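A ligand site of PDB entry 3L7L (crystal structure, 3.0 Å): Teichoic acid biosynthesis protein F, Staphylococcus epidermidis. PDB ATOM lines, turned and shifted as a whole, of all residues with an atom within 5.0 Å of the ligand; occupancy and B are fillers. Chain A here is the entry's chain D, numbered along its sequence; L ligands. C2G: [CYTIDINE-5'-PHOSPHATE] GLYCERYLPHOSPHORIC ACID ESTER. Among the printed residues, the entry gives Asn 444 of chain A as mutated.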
ATOM      1  N   PHE A 360      20.725 -25.009  10.874  1.00  0.00           N
ATOM      2  CA  PHE A 360      19.852 -25.122  12.025  1.00  0.00           C
ATOM      3  C   PHE A 360      20.584 -25.606  13.277  1.00  0.00           C
ATOM      4  O   PHE A 360      20.175 -26.587  13.911  1.00  0.00           O
ATOM      5  CB  PHE A 360      18.671 -26.030  11.700  1.00  0.00           C
ATOM      6  CG  PHE A 360      17.808 -25.506  10.597  1.00  0.00           C
ATOM      7  CD1 PHE A 360      17.355 -24.193  10.621  1.00  0.00           C
ATOM      8  CD2 PHE A 360      17.443 -26.326   9.528  1.00  0.00           C
ATOM      9  CE1 PHE A 360      16.571 -23.711   9.611  1.00  0.00           C
ATOM     10  CE2 PHE A 360      16.654 -25.828   8.502  1.00  0.00           C
ATOM     11  CZ  PHE A 360      16.218 -24.520   8.544  1.00  0.00           C
ATOM     12  N   TRP A 443      20.223 -17.134   6.335  1.00  0.00           N
ATOM     13  CA  TRP A 443      18.940 -17.166   7.019  1.00  0.00           C
ATOM     14  C   TRP A 443      18.066 -18.290   6.499  1.00  0.00           C
ATOM     15  O   TRP A 443      18.530 -19.191   5.817  1.00  0.00           O
ATOM     16  CB  TRP A 443      18.207 -15.832   6.952  1.00  0.00           C
ATOM     17  CG  TRP A 443      17.220 -15.643   8.079  1.00  0.00           C
ATOM     18  CD1 TRP A 443      15.909 -15.330   7.949  1.00  0.00           C
ATOM     19  CD2 TRP A 443      17.464 -15.774   9.486  1.00  0.00           C
ATOM     20  NE1 TRP A 443      15.316 -15.248   9.188  1.00  0.00           N
ATOM     21  CE2 TRP A 443      16.252 -15.517  10.149  1.00  0.00           C
ATOM     22  CE3 TRP A 443      18.592 -16.082  10.251  1.00  0.00           C
ATOM     23  CZ2 TRP A 443      16.133 -15.566  11.536  1.00  0.00           C
ATOM     24  CZ3 TRP A 443      18.464 -16.129  11.636  1.00  0.00           C
ATOM     25  CH2 TRP A 443      17.249 -15.863  12.263  1.00  0.00           C
ATOM     26  N   ASN A 444      16.785 -18.234   6.816  1.00  0.00           N
ATOM     27  CA  ASN A 444      15.981 -19.420   6.646  1.00  0.00           C
ATOM     28  C   ASN A 444      14.558 -19.147   6.212  1.00  0.00           C
ATOM     29  O   ASN A 444      13.658 -19.902   6.564  1.00  0.00           O
ATOM     30  CB  ASN A 444      15.998 -20.222   7.939  1.00  0.00           C
ATOM     31  CG  ASN A 444      15.582 -19.395   9.139  1.00  0.00           C
ATOM     32  OD1 ASN A 444      14.385 -19.145   9.346  1.00  0.00           O
ATOM     33  ND2 ASN A 444      16.571 -18.948   9.955  1.00  0.00           N
ATOM     34  N   GLY A 445      14.344 -18.080   5.441  1.00  0.00           N
ATOM     35  CA  GLY A 445      13.075 -17.852   4.789  1.00  0.00           C
ATOM     36  C   GLY A 445      12.599 -16.418   4.808  1.00  0.00           C
ATOM     37  O   GLY A 445      13.143 -15.593   5.513  1.00  0.00           O
ATOM     38  N   THR A 446      11.574 -16.126   4.025  1.00  0.00           N
ATOM     39  CA  THR A 446      10.976 -14.808   3.938  1.00  0.00           C
ATOM     40  C   THR A 446      10.033 -14.666   5.109  1.00  0.00           C
ATOM     41  O   THR A 446       9.141 -15.491   5.263  1.00  0.00           O
ATOM     42  CB  THR A 446      10.174 -14.662   2.643  1.00  0.00           C
ATOM     43  OG1 THR A 446      11.071 -14.599   1.526  1.00  0.00           O
ATOM     44  CG2 THR A 446       9.332 -13.422   2.659  1.00  0.00           C
ATOM     45  N   PRO A 447      10.229 -13.621   5.952  1.00  0.00           N
ATOM     46  CA  PRO A 447       9.557 -13.471   7.255  1.00  0.00           C
ATOM     47  C   PRO A 447       8.062 -13.205   7.167  1.00  0.00           C
ATOM     48  O   PRO A 447       7.574 -12.523   6.269  1.00  0.00           O
ATOM     49  CB  PRO A 447      10.240 -12.240   7.877  1.00  0.00           C
ATOM     50  CG  PRO A 447      11.364 -11.878   6.988  1.00  0.00           C
ATOM     51  CD  PRO A 447      11.063 -12.453   5.632  1.00  0.00           C
ATOM     52  N   LEU A 448       7.323 -13.757   8.110  1.00  0.00           N
ATOM     53  CA  LEU A 448       5.928 -13.388   8.238  1.00  0.00           C
ATOM     54  C   LEU A 448       5.726 -12.713   9.564  1.00  0.00           C
ATOM     55  O   LEU A 448       5.278 -11.591   9.606  1.00  0.00           O
ATOM     56  CB  LEU A 448       4.995 -14.587   8.075  1.00  0.00           C
ATOM     57  CG  LEU A 448       3.526 -14.177   8.083  1.00  0.00           C
ATOM     58  CD1 LEU A 448       3.243 -13.174   6.971  1.00  0.00           C
ATOM     59  CD2 LEU A 448       2.632 -15.379   7.933  1.00  0.00           C
ATOM     60  N   LEU A 451      10.422 -10.402  13.707  1.00  0.00           N
ATOM     61  CA  LEU A 451      11.528 -11.051  14.387  1.00  0.00           C
ATOM     62  C   LEU A 451      12.569 -10.048  14.808  1.00  0.00           C
ATOM     63  O   LEU A 451      12.401  -8.853  14.596  1.00  0.00           O
ATOM     64  CB  LEU A 451      12.209 -12.082  13.486  1.00  0.00           C
ATOM     65  CG  LEU A 451      12.317 -11.803  11.986  1.00  0.00           C
ATOM     66  CD1 LEU A 451      12.488 -10.320  11.699  1.00  0.00           C
ATOM     67  CD2 LEU A 451      13.453 -12.618  11.383  1.00  0.00           C
ATOM     68  N   PHE A 493      14.756  -7.043   6.599  1.00  0.00           N
ATOM     69  CA  PHE A 493      16.048  -7.376   7.170  1.00  0.00           C
ATOM     70  C   PHE A 493      16.759  -6.119   7.668  1.00  0.00           C
ATOM     71  O   PHE A 493      17.149  -6.024   8.831  1.00  0.00           O
ATOM     72  CB  PHE A 493      16.902  -8.139   6.166  1.00  0.00           C
ATOM     73  CG  PHE A 493      16.418  -9.539   5.911  1.00  0.00           C
ATOM     74  CD1 PHE A 493      15.466 -10.113   6.732  1.00  0.00           C
ATOM     75  CD2 PHE A 493      16.937 -10.292   4.870  1.00  0.00           C
ATOM     76  CE1 PHE A 493      15.021 -11.407   6.510  1.00  0.00           C
ATOM     77  CE2 PHE A 493      16.504 -11.595   4.629  1.00  0.00           C
ATOM     78  CZ  PHE A 493      15.543 -12.152   5.463  1.00  0.00           C
ATOM     79  N   ARG A 511      18.231 -23.029  -1.422  1.00  0.00           N
ATOM     80  CA  ARG A 511      17.498 -24.260  -1.228  1.00  0.00           C
ATOM     81  C   ARG A 511      16.336 -24.295  -2.187  1.00  0.00           C
ATOM     82  O   ARG A 511      15.743 -25.345  -2.431  1.00  0.00           O
ATOM     83  CB  ARG A 511      16.992 -24.383   0.194  1.00  0.00           C
ATOM     84  CG  ARG A 511      16.311 -23.140   0.718  1.00  0.00           C
ATOM     85  CD  ARG A 511      15.061 -23.507   1.492  1.00  0.00           C
ATOM     86  NE  ARG A 511      15.027 -22.878   2.811  1.00  0.00           N
ATOM     87  CZ  ARG A 511      14.196 -21.909   3.178  1.00  0.00           C
ATOM     88  NH1 ARG A 511      14.252 -21.407   4.407  1.00  0.00           N
ATOM     89  NH2 ARG A 511      13.312 -21.436   2.309  1.00  0.00           N
ATOM     90  N   ALA A 544       1.642 -28.346   6.777  1.00  0.00           N
ATOM     91  CA  ALA A 544       2.823 -27.904   7.504  1.00  0.00           C
ATOM     92  C   ALA A 544       2.452 -26.791   8.464  1.00  0.00           C
ATOM     93  O   ALA A 544       2.696 -25.615   8.193  1.00  0.00           O
ATOM     94  CB  ALA A 544       3.858 -27.417   6.511  1.00  0.00           C
ATOM     95  N   PRO A 545       1.856 -27.162   9.601  1.00  0.00           N
ATOM     96  CA  PRO A 545       1.564 -26.134  10.597  1.00  0.00           C
ATOM     97  C   PRO A 545       2.823 -25.382  10.988  1.00  0.00           C
ATOM     98  O   PRO A 545       3.918 -25.602  10.448  1.00  0.00           O
ATOM     99  CB  PRO A 545       1.055 -26.939  11.792  1.00  0.00           C
ATOM    100  CG  PRO A 545       0.504 -28.150  11.214  1.00  0.00           C
ATOM    101  CD  PRO A 545       1.358 -28.473  10.016  1.00  0.00           C
ATOM    102  N   THR A 546       2.679 -24.436  11.918  1.00  0.00           N
ATOM    103  CA  THR A 546       3.837 -23.879  12.574  1.00  0.00           C
ATOM    104  C   THR A 546       3.570 -24.019  14.030  1.00  0.00           C
ATOM    105  O   THR A 546       2.416 -24.154  14.444  1.00  0.00           O
ATOM    106  CB  THR A 546       4.159 -22.440  12.141  1.00  0.00           C
ATOM    107  OG1 THR A 546       4.987 -22.484  10.978  1.00  0.00           O
ATOM    108  CG2 THR A 546       4.928 -21.711  13.223  1.00  0.00           C
ATOM    109  N   TRP A 547       4.655 -23.977  14.790  1.00  0.00           N
ATOM    110  CA  TRP A 547       4.737 -24.477  16.160  1.00  0.00           C
ATOM    111  C   TRP A 547       3.893 -23.761  17.224  1.00  0.00           C
ATOM    112  O   TRP A 547       3.796 -22.529  17.254  1.00  0.00           O
ATOM    113  CB  TRP A 547       6.201 -24.511  16.555  1.00  0.00           C
ATOM    114  CG  TRP A 547       7.051 -23.716  15.591  1.00  0.00           C
ATOM    115  CD1 TRP A 547       7.170 -23.914  14.237  1.00  0.00           C
ATOM    116  CD2 TRP A 547       7.908 -22.596  15.908  1.00  0.00           C
ATOM    117  NE1 TRP A 547       8.037 -22.987  13.704  1.00  0.00           N
ATOM    118  CE2 TRP A 547       8.507 -22.174  14.705  1.00  0.00           C
ATOM    119  CE3 TRP A 547       8.230 -21.921  17.094  1.00  0.00           C
ATOM    120  CZ2 TRP A 547       9.397 -21.097  14.655  1.00  0.00           C
ATOM    121  CZ3 TRP A 547       9.108 -20.856  17.041  1.00  0.00           C
ATOM    122  CH2 TRP A 547       9.690 -20.466  15.829  1.00  0.00           C
ATOM    123  N   ARG A 582       3.938 -32.530   7.981  1.00  0.00           N
ATOM    124  CA  ARG A 582       5.283 -32.154   8.399  1.00  0.00           C
ATOM    125  C   ARG A 582       5.216 -31.283   9.623  1.00  0.00           C
ATOM    126  O   ARG A 582       5.111 -30.067   9.500  1.00  0.00           O
ATOM    127  CB  ARG A 582       6.021 -31.410   7.295  1.00  0.00           C
ATOM    128  CG  ARG A 582       7.431 -31.105   7.668  1.00  0.00           C
ATOM    129  CD  ARG A 582       8.267 -30.938   6.439  1.00  0.00           C
ATOM    130  NE  ARG A 582       9.668 -30.717   6.754  1.00  0.00           N
ATOM    131  CZ  ARG A 582      10.558 -31.683   6.943  1.00  0.00           C
ATOM    132  NH1 ARG A 582      10.206 -32.965   6.860  1.00  0.00           N
ATOM    133  NH2 ARG A 582      11.813 -31.363   7.211  1.00  0.00           N
ATOM    134  N   MET A 583       5.283 -31.913  10.799  1.00  0.00           N
ATOM    135  CA  MET A 583       4.972 -31.256  12.063  1.00  0.00           C
ATOM    136  C   MET A 583       6.212 -30.820  12.807  1.00  0.00           C
ATOM    137  O   MET A 583       7.209 -30.422  12.212  1.00  0.00           O
ATOM    138  CB  MET A 583       4.192 -32.204  12.963  1.00  0.00           C
ATOM    139  CG  MET A 583       3.295 -33.174  12.236  1.00  0.00           C
ATOM    140  SD  MET A 583       1.715 -32.460  11.796  1.00  0.00           S
ATOM    141  CE  MET A 583       1.403 -31.451  13.234  1.00  0.00           C
ATOM    142  N   VAL A 609      13.004 -30.505   2.480  1.00  0.00           N
ATOM    143  CA  VAL A 609      11.617 -30.061   2.422  1.00  0.00           C
ATOM    144  C   VAL A 609      11.266 -29.573   1.020  1.00  0.00           C
ATOM    145  O   VAL A 609      10.098 -29.569   0.626  1.00  0.00           O
ATOM    146  CB  VAL A 609      11.375 -28.936   3.433  1.00  0.00           C
ATOM    147  CG1 VAL A 609      11.606 -27.610   2.778  1.00  0.00           C
ATOM    148  CG2 VAL A 609       9.984 -29.012   3.970  1.00  0.00           C
ATOM    149  N   TYR A 623       0.631 -19.803   9.587  1.00  0.00           N
ATOM    150  CA  TYR A 623       1.484 -18.664   9.716  1.00  0.00           C
ATOM    151  C   TYR A 623       2.899 -19.154   9.608  1.00  0.00           C
ATOM    152  O   TYR A 623       3.543 -19.337  10.625  1.00  0.00           O
ATOM    153  CB  TYR A 623       1.300 -18.046  11.096  1.00  0.00           C
ATOM    154  CG  TYR A 623      -0.071 -18.266  11.689  1.00  0.00           C
ATOM    155  CD1 TYR A 623      -0.217 -18.857  12.936  1.00  0.00           C
ATOM    156  CD2 TYR A 623      -1.208 -17.892  11.001  1.00  0.00           C
ATOM    157  CE1 TYR A 623      -1.445 -19.065  13.496  1.00  0.00           C
ATOM    158  CE2 TYR A 623      -2.456 -18.103  11.551  1.00  0.00           C
ATOM    159  CZ  TYR A 623      -2.569 -18.694  12.796  1.00  0.00           C
ATOM    160  OH  TYR A 623      -3.800 -18.901  13.370  1.00  0.00           O
ATOM    161  N   SER A 624       3.377 -19.364   8.387  1.00  0.00           N
ATOM    162  CA  SER A 624       4.690 -19.966   8.184  1.00  0.00           C
ATOM    163  C   SER A 624       5.399 -19.380   6.983  1.00  0.00           C
ATOM    164  O   SER A 624       4.767 -18.954   6.036  1.00  0.00           O
ATOM    165  CB  SER A 624       4.567 -21.478   7.978  1.00  0.00           C
ATOM    166  OG  SER A 624       5.766 -22.011   7.445  1.00  0.00           O
ATOM    167  N   SER A 625       6.722 -19.382   7.031  1.00  0.00           N
ATOM    168  CA  SER A 625       7.472 -18.800   5.945  1.00  0.00           C
ATOM    169  C   SER A 625       7.601 -19.788   4.806  1.00  0.00           C
ATOM    170  O   SER A 625       8.097 -19.433   3.745  1.00  0.00           O
ATOM    171  CB  SER A 625       8.853 -18.338   6.390  1.00  0.00           C
ATOM    172  OG  SER A 625       9.840 -19.299   6.036  1.00  0.00           O
ATOM    173  N   VAL A 626       7.154 -21.041   5.006  1.00  0.00           N
ATOM    174  CA  VAL A 626       7.202 -21.997   3.896  1.00  0.00           C
ATOM    175  C   VAL A 626       6.206 -21.574   2.829  1.00  0.00           C
ATOM    176  O   VAL A 626       6.299 -21.996   1.681  1.00  0.00           O
ATOM    177  CB  VAL A 626       6.928 -23.489   4.280  1.00  0.00           C
ATOM    178  CG1 VAL A 626       7.638 -23.867   5.556  1.00  0.00           C
ATOM    179  CG2 VAL A 626       5.462 -23.735   4.427  1.00  0.00           C
ATOM    180  N   ASP A 629       8.226 -19.933   0.036  1.00  0.00           N
ATOM    181  CA  ASP A 629       9.008 -20.875  -0.734  1.00  0.00           C
ATOM    182  C   ASP A 629       8.099 -21.604  -1.725  1.00  0.00           C
ATOM    183  O   ASP A 629       8.372 -21.681  -2.911  1.00  0.00           O
ATOM    184  CB  ASP A 629       9.700 -21.864   0.203  1.00  0.00           C
ATOM    185  CG  ASP A 629      10.656 -21.181   1.168  1.00  0.00           C
ATOM    186  OD1 ASP A 629      10.637 -21.510   2.389  1.00  0.00           O
ATOM    187  OD2 ASP A 629      11.442 -20.325   0.708  1.00  0.00           O
HETATM  188  N1  C2G L   1      10.187 -25.655   7.563  1.00  0.00           N
HETATM  189  C2  C2G L   1       9.858 -27.161   7.529  1.00  0.00           C
HETATM  190  N3  C2G L   1       8.557 -27.656   8.067  1.00  0.00           N
HETATM  191  C4  C2G L   1       7.565 -26.722   8.658  1.00  0.00           C
HETATM  192  C5  C2G L   1       7.883 -25.250   8.711  1.00  0.00           C
HETATM  193  C6  C2G L   1       9.198 -24.743   8.162  1.00  0.00           C
HETATM  194  O2  C2G L   1      10.758 -28.090   6.995  1.00  0.00           O
HETATM  195  N4  C2G L   1       6.303 -27.182   9.202  1.00  0.00           N
HETATM  196  C1' C2G L   1      11.444 -25.049   7.059  1.00  0.00           C
HETATM  197  C2' C2G L   1      11.204 -24.290   5.736  1.00  0.00           C
HETATM  198  O2' C2G L   1      12.226 -24.512   4.781  1.00  0.00           O
HETATM  199  C3' C2G L   1      11.085 -22.829   6.131  1.00  0.00           C
HETATM  200  C4' C2G L   1      11.882 -22.713   7.436  1.00  0.00           C
HETATM  201  O4' C2G L   1      11.939 -24.059   8.026  1.00  0.00           O
HETATM  202  O3' C2G L   1      11.537 -21.936   5.133  1.00  0.00           O
HETATM  203  C5' C2G L   1      11.217 -21.724   8.433  1.00  0.00           C
HETATM  204  O5' C2G L   1       9.809 -21.657   8.298  1.00  0.00           O
HETATM  205  PA  C2G L   1       8.879 -21.211   9.617  1.00  0.00           P
HETATM  206  O1A C2G L   1       7.650 -22.275   9.896  1.00  0.00           O
HETATM  207  O2A C2G L   1       8.328 -19.858   9.481  1.00  0.00           O
HETATM  208  O3A C2G L   1       9.908 -21.263  10.921  1.00  0.00           O
HETATM  209  PB  C2G L   1      10.823 -19.964  11.381  1.00  0.00           P
HETATM  210  O1B C2G L   1      12.247 -20.567  11.972  1.00  0.00           O
HETATM  211  O2B C2G L   1      10.080 -19.211  12.390  1.00  0.00           O
HETATM  212  O3B C2G L   1      11.173 -18.955  10.105  1.00  0.00           O
HETATM  213  O1G C2G L   1      12.723 -15.403   8.222  1.00  0.00           O
HETATM  214  C1G C2G L   1      11.471 -15.981   8.432  1.00  0.00           C
HETATM  215  C2G C2G L   1      11.540 -16.609   9.831  1.00  0.00           C
HETATM  216  O2G C2G L   1      12.830 -17.114  10.010  1.00  0.00           O
HETATM  217  C3G C2G L   1      10.494 -17.739   9.927  1.00  0.00           C
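NH1 of Arg 511 lies within hydrogen-bond range of O of Asn 444 (2.7 Å). The side-chain carboxylate of Asp 629 is in salt-bridge range of the guanidinium group of Arg 511 (2.7 Å). OG1 of Thr 546 is in hydrogen-bond range of O of Tyr 623, at 3.5 Å. N of Val 626 sits at hydrogen-bond distance from OG of Ser 624.
C of Thr 446 touches C1G of the ligand, 3.9 Å away. Pro 447 touches the ligand. Ala 544 touches the ligand. Trp 547 touches the ligand. CG2 of Val 609 touches O2 of the ligand, 3.3 Å away. Val 626 touches the ligand. Within 4 Å of the ligand: Trp 443, Asn 444, Gly 445, Thr 446, Pro 447, Arg 511, Ala 544, Pro 545, Thr 546, Trp 547, Arg 582, Val 609, Ser 624, Ser 625, Val 626 and Asp 629. The nearest printed residue that does not touch the ligand is Leu 451 (4.3 Å).
O of Asn 444 lies within hydrogen-bond range of O3' of the ligand (3.3 Å). The side-chain amide oxygen (OD1) of Asn 444 is in hydrogen-bond range of an oxygen (O2G) of the ligand (2.6 Å). An oxygen (O1G) of the ligand sits at hydrogen-bond distance from the backbone carbonyl oxygen of Gly 445 (2.7 Å). The indole nitrogen (NE1) of Trp 443 is in hydrogen-bond range of an oxygen (O1G) of the ligand (2.8 Å). N4 of the ligand lies within hydrogen-bond range of O of Arg 582 (3.1 Å). The guanidinium group (NE) of Arg 582 sits at hydrogen-bond distance from an oxygen (O2) of the ligand. The guanidinium group of Arg 511 lies within hydrogen-bond range of an oxygen (O3') of the ligand (2.9 Å). OG1 of Thr 546 is in hydrogen-bond range of O1A of the ligand. An oxygen (O3') of the ligand is in hydrogen-bond range of the side-chain carboxylate (OD1) of Asp 629 (2.9 Å). N of Ser 625 sits at hydrogen-bond distance from O2A of the ligand. O3' of the ligand is in hydrogen-bond range of OG of Ser 625 (3.3 Å). An oxygen (O1A) of the ligand is in hydrogen-bond range of the side-chain hydroxyl (OG) of Ser 624, at 3.1 Å. O of Pro 545 is in hydrogen-bond range of N4 of the ligand, at 3.1 Å.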
